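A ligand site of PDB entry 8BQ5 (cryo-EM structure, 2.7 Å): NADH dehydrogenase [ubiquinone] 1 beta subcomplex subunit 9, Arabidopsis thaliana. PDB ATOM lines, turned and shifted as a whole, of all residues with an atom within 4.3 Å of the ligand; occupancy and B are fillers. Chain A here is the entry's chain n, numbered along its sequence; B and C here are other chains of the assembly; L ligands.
The backbone NH (N) of Ser 79 of chain B lies close to an oxygen (O2) of the ligand.
An oxygen (O2) of the ligand sits at hydrogen-bond distance from the side-chain hydroxyl of Ser 79 of chain B (2.8 Å).
O of Gln 56 lies within hydrogen-bond range of O5 of the ligand (2.9 Å).
The guanidinium group (NH2) of Arg 13 sits at hydrogen-bond distance from an oxygen (O6) of the ligand (3.2 Å).
N2 of the ligand sits at hydrogen-bond distance from O of Asn 55.
The side-chain amino group of Lys 17 lies close to an oxygen (O6) of the ligand (3.5 Å).
An oxygen (O3) of the ligand is in salt-bridge range of the guanidinium group (NH1) of Arg 21.
The indole nitrogen (NE1) of Trp 78 is in hydrogen-bond range of the side-chain carboxylate (OE1) of Glu 74, at 2.8 Å.
Residues that only touch the ligand: Gln 547 of chain C (3.3 Å), Val 58 (3.5 Å), Val 20 (3.6 Å), Leu 67 (3.6 Å), Asp 30 (3.6 Å), Phe 52 (3.7 Å), Gly 71 (3.7 Å), Trp 78 (3.8 Å), Lys 51 (3.9 Å) and Ile 64 (3.98 Å).
Hydrophobic or aromatic side chains that line the ligand: Val 20, Phe 52, Ile 64, Leu 67 and Trp 78.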
ATOM      1  N   ARG A  13     -24.303  23.272 -37.937  1.00  0.00           N
ATOM      2  CA  ARG A  13     -23.961  24.110 -36.791  1.00  0.00           C
ATOM      3  C   ARG A  13     -25.011  24.018 -35.692  1.00  0.00           C
ATOM      4  O   ARG A  13     -24.664  24.167 -34.514  1.00  0.00           O
ATOM      5  CB  ARG A  13     -23.767  25.557 -37.239  1.00  0.00           C
ATOM      6  CG  ARG A  13     -22.506  25.771 -38.053  1.00  0.00           C
ATOM      7  CD  ARG A  13     -21.313  26.067 -37.171  1.00  0.00           C
ATOM      8  NE  ARG A  13     -21.627  26.995 -36.095  1.00  0.00           N
ATOM      9  CZ  ARG A  13     -21.566  26.705 -34.807  1.00  0.00           C
ATOM     10  NH1 ARG A  13     -21.217  25.497 -34.390  1.00  0.00           N
ATOM     11  NH2 ARG A  13     -21.868  27.641 -33.915  1.00  0.00           N
ATOM     12  N   LYS A  17     -24.419  23.108 -31.779  1.00  0.00           N
ATOM     13  CA  LYS A  17     -24.971  23.860 -30.656  1.00  0.00           C
ATOM     14  C   LYS A  17     -25.637  22.931 -29.658  1.00  0.00           C
ATOM     15  O   LYS A  17     -25.489  23.098 -28.446  1.00  0.00           O
ATOM     16  CB  LYS A  17     -25.948  24.919 -31.158  1.00  0.00           C
ATOM     17  CG  LYS A  17     -25.302  26.126 -31.787  1.00  0.00           C
ATOM     18  CD  LYS A  17     -26.343  27.174 -32.163  1.00  0.00           C
ATOM     19  CE  LYS A  17     -25.732  28.264 -33.012  1.00  0.00           C
ATOM     20  NZ  LYS A  17     -24.771  27.685 -33.978  1.00  0.00           N
ATOM     21  N   VAL A  20     -23.124  21.103 -27.427  1.00  0.00           N
ATOM     22  CA  VAL A  20     -22.485  21.975 -26.446  1.00  0.00           C
ATOM     23  C   VAL A  20     -23.446  22.309 -25.309  1.00  0.00           C
ATOM     24  O   VAL A  20     -23.059  22.364 -24.140  1.00  0.00           O
ATOM     25  CB  VAL A  20     -21.949  23.240 -27.131  1.00  0.00           C
ATOM     26  CG1 VAL A  20     -21.447  24.246 -26.109  1.00  0.00           C
ATOM     27  CG2 VAL A  20     -20.840  22.883 -28.107  1.00  0.00           C
ATOM     28  N   ARG A  21     -24.712  22.550 -25.648  1.00  0.00           N
ATOM     29  CA  ARG A  21     -25.701  22.888 -24.624  1.00  0.00           C
ATOM     30  C   ARG A  21     -25.919  21.725 -23.663  1.00  0.00           C
ATOM     31  O   ARG A  21     -26.060  21.922 -22.459  1.00  0.00           O
ATOM     32  CB  ARG A  21     -27.008  23.297 -25.288  1.00  0.00           C
ATOM     33  CG  ARG A  21     -26.945  24.607 -26.035  1.00  0.00           C
ATOM     34  CD  ARG A  21     -28.282  25.321 -25.978  1.00  0.00           C
ATOM     35  NE  ARG A  21     -29.358  24.536 -26.576  1.00  0.00           N
ATOM     36  CZ  ARG A  21     -29.538  24.364 -27.870  1.00  0.00           C
ATOM     37  NH1 ARG A  21     -28.716  24.896 -28.766  1.00  0.00           N
ATOM     38  NH2 ARG A  21     -30.572  23.649 -28.291  1.00  0.00           N
ATOM     39  N   LEU A  23     -23.694  19.302 -23.103  1.00  0.00           N
ATOM     40  CA  LEU A  23     -22.456  19.131 -22.354  1.00  0.00           C
ATOM     41  C   LEU A  23     -22.388  20.116 -21.190  1.00  0.00           C
ATOM     42  O   LEU A  23     -21.925  19.777 -20.091  1.00  0.00           O
ATOM     43  CB  LEU A  23     -21.260  19.295 -23.282  1.00  0.00           C
ATOM     44  CG  LEU A  23     -19.901  19.163 -22.591  1.00  0.00           C
ATOM     45  CD1 LEU A  23     -19.788  17.815 -21.923  1.00  0.00           C
ATOM     46  CD2 LEU A  23     -18.785  19.351 -23.600  1.00  0.00           C
ATOM     47  N   ALA A  27     -22.289  18.935 -17.282  1.00  0.00           N
ATOM     48  CA  ALA A  27     -21.162  19.380 -16.480  1.00  0.00           C
ATOM     49  C   ALA A  27     -21.624  20.193 -15.284  1.00  0.00           C
ATOM     50  O   ALA A  27     -21.019  20.131 -14.198  1.00  0.00           O
ATOM     51  CB  ALA A  27     -20.198  20.195 -17.339  1.00  0.00           C
ATOM     52  N   ASP A  30     -22.930  17.747 -12.735  1.00  0.00           N
ATOM     53  CA  ASP A  30     -21.802  17.008 -12.132  1.00  0.00           C
ATOM     54  C   ASP A  30     -21.097  17.900 -11.104  1.00  0.00           C
ATOM     55  O   ASP A  30     -20.583  17.355 -10.132  1.00  0.00           O
ATOM     56  CB  ASP A  30     -20.794  16.560 -13.194  1.00  0.00           C
ATOM     57  CG  ASP A  30     -19.899  15.454 -12.695  1.00  0.00           C
ATOM     58  OD1 ASP A  30     -18.667  15.652 -12.683  1.00  0.00           O
ATOM     59  OD2 ASP A  30     -20.443  14.415 -12.299  1.00  0.00           O
ATOM     60  N   LYS A  51     -15.328  28.551 -18.538  1.00  0.00           N
ATOM     61  CA  LYS A  51     -14.560  27.718 -19.447  1.00  0.00           C
ATOM     62  C   LYS A  51     -15.255  27.569 -20.786  1.00  0.00           C
ATOM     63  O   LYS A  51     -14.615  27.456 -21.833  1.00  0.00           O
ATOM     64  CB  LYS A  51     -14.312  26.352 -18.806  1.00  0.00           C
ATOM     65  CG  LYS A  51     -13.424  25.414 -19.615  1.00  0.00           C
ATOM     66  CD  LYS A  51     -12.158  25.076 -18.851  1.00  0.00           C
ATOM     67  CE  LYS A  51     -12.464  24.711 -17.403  1.00  0.00           C
ATOM     68  NZ  LYS A  51     -13.313  23.487 -17.283  1.00  0.00           N
ATOM     69  N   PHE A  52     -16.591  27.559 -20.770  1.00  0.00           N
ATOM     70  CA  PHE A  52     -17.345  27.585 -22.020  1.00  0.00           C
ATOM     71  C   PHE A  52     -17.309  28.975 -22.656  1.00  0.00           C
ATOM     72  O   PHE A  52     -17.434  29.109 -23.878  1.00  0.00           O
ATOM     73  CB  PHE A  52     -18.791  27.156 -21.788  1.00  0.00           C
ATOM     74  CG  PHE A  52     -19.011  25.677 -21.860  1.00  0.00           C
ATOM     75  CD1 PHE A  52     -18.716  24.857 -20.779  1.00  0.00           C
ATOM     76  CD2 PHE A  52     -19.516  25.092 -23.014  1.00  0.00           C
ATOM     77  CE1 PHE A  52     -18.915  23.493 -20.847  1.00  0.00           C
ATOM     78  CE2 PHE A  52     -19.716  23.728 -23.082  1.00  0.00           C
ATOM     79  CZ  PHE A  52     -19.412  22.926 -21.991  1.00  0.00           C
ATOM     80  N   ASN A  55     -14.164  29.812 -25.264  1.00  0.00           N
ATOM     81  CA  ASN A  55     -14.278  29.432 -26.663  1.00  0.00           C
ATOM     82  C   ASN A  55     -15.624  29.803 -27.264  1.00  0.00           C
ATOM     83  O   ASN A  55     -15.968  29.297 -28.344  1.00  0.00           O
ATOM     84  CB  ASN A  55     -14.053  27.919 -26.811  1.00  0.00           C
ATOM     85  CG  ASN A  55     -12.756  27.466 -26.188  1.00  0.00           C
ATOM     86  OD1 ASN A  55     -12.730  26.997 -25.049  1.00  0.00           O
ATOM     87  ND2 ASN A  55     -11.663  27.592 -26.937  1.00  0.00           N
ATOM     88  N   GLN A  56     -16.383  30.678 -26.618  1.00  0.00           N
ATOM     89  CA  GLN A  56     -17.744  30.980 -27.052  1.00  0.00           C
ATOM     90  C   GLN A  56     -17.796  31.661 -28.410  1.00  0.00           C
ATOM     91  O   GLN A  56     -18.872  31.745 -29.017  1.00  0.00           O
ATOM     92  CB  GLN A  56     -18.447  31.866 -26.016  1.00  0.00           C
ATOM     93  CG  GLN A  56     -17.984  33.311 -26.039  1.00  0.00           C
ATOM     94  CD  GLN A  56     -18.671  34.183 -25.009  1.00  0.00           C
ATOM     95  OE1 GLN A  56     -18.953  33.744 -23.890  1.00  0.00           O
ATOM     96  NE2 GLN A  56     -18.947  35.429 -25.369  1.00  0.00           N
ATOM     97  N   VAL A  58     -15.485  31.003 -31.087  1.00  0.00           N
ATOM     98  CA  VAL A  58     -14.795  30.279 -32.153  1.00  0.00           C
ATOM     99  C   VAL A  58     -15.749  30.063 -33.311  1.00  0.00           C
ATOM    100  O   VAL A  58     -16.906  29.655 -33.131  1.00  0.00           O
ATOM    101  CB  VAL A  58     -14.237  28.952 -31.607  1.00  0.00           C
ATOM    102  CG1 VAL A  58     -13.766  28.069 -32.754  1.00  0.00           C
ATOM    103  CG2 VAL A  58     -13.097  29.217 -30.634  1.00  0.00           C
ATOM    104  N   ILE A  64     -14.638  23.342 -33.745  1.00  0.00           N
ATOM    105  CA  ILE A  64     -15.754  23.082 -32.838  1.00  0.00           C
ATOM    106  C   ILE A  64     -15.878  21.596 -32.572  1.00  0.00           C
ATOM    107  O   ILE A  64     -16.074  21.164 -31.421  1.00  0.00           O
ATOM    108  CB  ILE A  64     -17.063  23.662 -33.425  1.00  0.00           C
ATOM    109  CG1 ILE A  64     -17.022  25.186 -33.384  1.00  0.00           C
ATOM    110  CG2 ILE A  64     -18.254  23.159 -32.636  1.00  0.00           C
ATOM    111  CD1 ILE A  64     -17.996  25.840 -34.345  1.00  0.00           C
ATOM    112  N   LEU A  67     -13.177  20.639 -30.170  1.00  0.00           N
ATOM    113  CA  LEU A  67     -13.455  21.168 -28.840  1.00  0.00           C
ATOM    114  C   LEU A  67     -14.572  20.392 -28.166  1.00  0.00           C
ATOM    115  O   LEU A  67     -14.530  20.152 -26.950  1.00  0.00           O
ATOM    116  CB  LEU A  67     -13.797  22.657 -28.906  1.00  0.00           C
ATOM    117  CG  LEU A  67     -12.640  23.607 -29.197  1.00  0.00           C
ATOM    118  CD1 LEU A  67     -13.147  25.039 -29.334  1.00  0.00           C
ATOM    119  CD2 LEU A  67     -11.595  23.508 -28.106  1.00  0.00           C
ATOM    120  N   ILE A  68     -15.596  19.990 -28.916  1.00  0.00           N
ATOM    121  CA  ILE A  68     -16.658  19.174 -28.350  1.00  0.00           C
ATOM    122  C   ILE A  68     -16.094  17.826 -27.903  1.00  0.00           C
ATOM    123  O   ILE A  68     -16.264  17.421 -26.753  1.00  0.00           O
ATOM    124  CB  ILE A  68     -17.813  19.002 -29.347  1.00  0.00           C
ATOM    125  CG1 ILE A  68     -18.511  20.333 -29.594  1.00  0.00           C
ATOM    126  CG2 ILE A  68     -18.812  17.982 -28.850  1.00  0.00           C
ATOM    127  CD1 ILE A  68     -19.495  20.298 -30.740  1.00  0.00           C
ATOM    128  N   GLY A  71     -14.134  18.002 -24.913  1.00  0.00           N
ATOM    129  CA  GLY A  71     -14.990  18.291 -23.780  1.00  0.00           C
ATOM    130  C   GLY A  71     -15.773  17.080 -23.301  1.00  0.00           C
ATOM    131  O   GLY A  71     -15.878  16.834 -22.095  1.00  0.00           O
ATOM    132  N   GLU A  74     -13.717  14.795 -21.327  1.00  0.00           N
ATOM    133  CA  GLU A  74     -13.419  15.374 -20.017  1.00  0.00           C
ATOM    134  C   GLU A  74     -14.554  15.091 -19.030  1.00  0.00           C
ATOM    135  O   GLU A  74     -14.303  14.620 -17.917  1.00  0.00           O
ATOM    136  CB  GLU A  74     -13.198  16.886 -20.154  1.00  0.00           C
ATOM    137  CG  GLU A  74     -11.832  17.287 -20.698  1.00  0.00           C
ATOM    138  CD  GLU A  74     -10.704  17.038 -19.710  1.00  0.00           C
ATOM    139  OE1 GLU A  74     -10.986  16.745 -18.533  1.00  0.00           O
ATOM    140  OE2 GLU A  74      -9.529  17.137 -20.122  1.00  0.00           O
ATOM    141  N   TYR A  75     -15.776  15.444 -19.410  1.00  0.00           N
ATOM    142  CA  TYR A  75     -16.943  15.129 -18.536  1.00  0.00           C
ATOM    143  C   TYR A  75     -16.911  13.633 -18.222  1.00  0.00           C
ATOM    144  O   TYR A  75     -17.011  13.295 -17.036  1.00  0.00           O
ATOM    145  CB  TYR A  75     -18.256  15.533 -19.206  1.00  0.00           C
ATOM    146  CG  TYR A  75     -19.484  15.023 -18.490  1.00  0.00           C
ATOM    147  CD1 TYR A  75     -20.311  14.081 -19.087  1.00  0.00           C
ATOM    148  CD2 TYR A  75     -19.813  15.469 -17.225  1.00  0.00           C
ATOM    149  CE1 TYR A  75     -21.437  13.599 -18.433  1.00  0.00           C
ATOM    150  CE2 TYR A  75     -20.930  15.005 -16.561  1.00  0.00           C
ATOM    151  CZ  TYR A  75     -21.751  14.064 -17.166  1.00  0.00           C
ATOM    152  OH  TYR A  75     -22.858  13.604 -16.518  1.00  0.00           O
ATOM    153  N   TRP A  78     -13.993  12.848 -15.531  1.00  0.00           N
ATOM    154  CA  TRP A  78     -14.109  13.352 -14.128  1.00  0.00           C
ATOM    155  C   TRP A  78     -15.569  13.363 -13.652  1.00  0.00           C
ATOM    156  O   TRP A  78     -15.848  14.058 -12.659  1.00  0.00           O
ATOM    157  CB  TRP A  78     -13.437  14.721 -13.950  1.00  0.00           C
ATOM    158  CG  TRP A  78     -12.114  14.814 -14.632  1.00  0.00           C
ATOM    159  CD1 TRP A  78     -11.878  15.278 -15.896  1.00  0.00           C
ATOM    160  CD2 TRP A  78     -10.841  14.427 -14.107  1.00  0.00           C
ATOM    161  NE1 TRP A  78     -10.537  15.198 -16.184  1.00  0.00           N
ATOM    162  CE2 TRP A  78      -9.878  14.692 -15.099  1.00  0.00           C
ATOM    163  CE3 TRP A  78     -10.413  13.886 -12.886  1.00  0.00           C
ATOM    164  CZ2 TRP A  78      -8.519  14.438 -14.921  1.00  0.00           C
ATOM    165  CZ3 TRP A  78      -9.075  13.643 -12.707  1.00  0.00           C
ATOM    166  CH2 TRP A  78      -8.136  13.906 -13.703  1.00  0.00           C
ATOM    167  N   GLN B  72     -34.093  33.868 -25.563  1.00  0.00           N
ATOM    168  CA  GLN B  72     -33.086  34.363 -26.496  1.00  0.00           C
ATOM    169  C   GLN B  72     -33.612  35.412 -27.463  1.00  0.00           C
ATOM    170  O   GLN B  72     -32.868  35.857 -28.334  1.00  0.00           O
ATOM    171  CB  GLN B  72     -32.473  33.201 -27.280  1.00  0.00           C
ATOM    172  CG  GLN B  72     -31.428  32.412 -26.512  1.00  0.00           C
ATOM    173  CD  GLN B  72     -30.340  31.878 -27.422  1.00  0.00           C
ATOM    174  OE1 GLN B  72     -30.374  30.718 -27.832  1.00  0.00           O
ATOM    175  NE2 GLN B  72     -29.374  32.727 -27.751  1.00  0.00           N
ATOM    176  N   SER B  79     -27.697  31.088 -24.907  1.00  0.00           N
ATOM    177  CA  SER B  79     -28.335  29.803 -24.655  1.00  0.00           C
ATOM    178  C   SER B  79     -27.787  29.115 -23.406  1.00  0.00           C
ATOM    179  O   SER B  79     -28.534  28.401 -22.722  1.00  0.00           O
ATOM    180  CB  SER B  79     -28.172  28.877 -25.852  1.00  0.00           C
ATOM    181  OG  SER B  79     -26.921  28.217 -25.829  1.00  0.00           O
ATOM    182  N   GLN C 547     -10.949  16.338  -8.909  1.00  0.00           N
ATOM    183  CA  GLN C 547     -11.379  16.749 -10.235  1.00  0.00           C
ATOM    184  C   GLN C 547     -10.235  17.077 -11.181  1.00  0.00           C
ATOM    185  O   GLN C 547     -10.471  17.208 -12.390  1.00  0.00           O
ATOM    186  CB  GLN C 547     -12.315  17.963 -10.142  1.00  0.00           C
ATOM    187  CG  GLN C 547     -13.770  17.594  -9.949  1.00  0.00           C
ATOM    188  CD  GLN C 547     -14.714  18.657 -10.477  1.00  0.00           C
ATOM    189  OE1 GLN C 547     -14.658  19.016 -11.663  1.00  0.00           O
ATOM    190  NE2 GLN C 547     -15.590  19.155  -9.621  1.00  0.00           N
HETATM  191  O1  LIG L   1     -15.783  24.962 -25.019  1.00  0.00           O
HETATM  192  C1  LIG L   1     -15.980  17.479 -14.269  1.00  0.00           C
HETATM  193  O2  LIG L   1     -26.037  30.079 -27.686  1.00  0.00           O
HETATM  194  C2  LIG L   1     -16.559  17.955 -15.590  1.00  0.00           C
HETATM  195  C3  LIG L   1     -15.445  18.530 -16.471  1.00  0.00           C
HETATM  196  C4  LIG L   1     -15.964  19.778 -17.180  1.00  0.00           C
HETATM  197  O3  LIG L   1     -27.317  28.228 -28.742  1.00  0.00           O
HETATM  198  C5  LIG L   1     -16.133  19.506 -18.674  1.00  0.00           C
HETATM  199  C6  LIG L   1     -15.534  20.679 -19.450  1.00  0.00           C
HETATM  200  C7  LIG L   1     -16.109  20.717 -20.861  1.00  0.00           C
HETATM  201  C8  LIG L   1     -15.113  21.415 -21.788  1.00  0.00           C
HETATM  202  C9  LIG L   1     -15.431  22.906 -21.850  1.00  0.00           C
HETATM  203  C10 LIG L   1     -14.669  23.507 -23.036  1.00  0.00           C
HETATM  204  C11 LIG L   1     -15.090  22.814 -24.331  1.00  0.00           C
HETATM  205  C12 LIG L   1     -15.878  23.795 -25.203  1.00  0.00           C
HETATM  206  C13 LIG L   1     -23.892  28.277 -27.548  1.00  0.00           C
HETATM  207  C14 LIG L   1     -22.467  28.281 -28.102  1.00  0.00           C
HETATM  208  C15 LIG L   1     -21.465  28.419 -26.957  1.00  0.00           C
HETATM  209  C16 LIG L   1     -22.246  26.951 -28.814  1.00  0.00           C
HETATM  210  C17 LIG L   1     -22.340  29.474 -29.066  1.00  0.00           C
HETATM  211  C18 LIG L   1     -22.069  29.041 -30.522  1.00  0.00           C
HETATM  212  C19 LIG L   1     -19.516  28.826 -30.312  1.00  0.00           C
HETATM  213  C20 LIG L   1     -18.564  27.718 -30.733  1.00  0.00           C
HETATM  214  C21 LIG L   1     -18.618  26.626 -29.674  1.00  0.00           C
HETATM  215  C22 LIG L   1     -17.777  25.524 -27.610  1.00  0.00           C
HETATM  216  C23 LIG L   1     -16.811  24.381 -27.910  1.00  0.00           C
HETATM  217  N1  LIG L   1     -20.754  28.752 -31.072  1.00  0.00           N
HETATM  218  N2  LIG L   1     -17.645  26.575 -28.605  1.00  0.00           N
HETATM  219  O4  LIG L   1     -24.763  28.049 -28.619  1.00  0.00           O
HETATM  220  O5  LIG L   1     -21.392  30.401 -28.589  1.00  0.00           O
HETATM  221  O6  LIG L   1     -23.007  28.946 -31.241  1.00  0.00           O
HETATM  222  O7  LIG L   1     -19.492  25.819 -29.712  1.00  0.00           O
HETATM  223  P1  LIG L   1     -26.059  29.046 -28.796  1.00  0.00           P
HETATM  224  S1  LIG L   1     -16.924  23.189 -26.550  1.00  0.00           S
HETATM  225  O8  LIG L   1     -25.987  29.767 -30.126  1.00  0.00           O
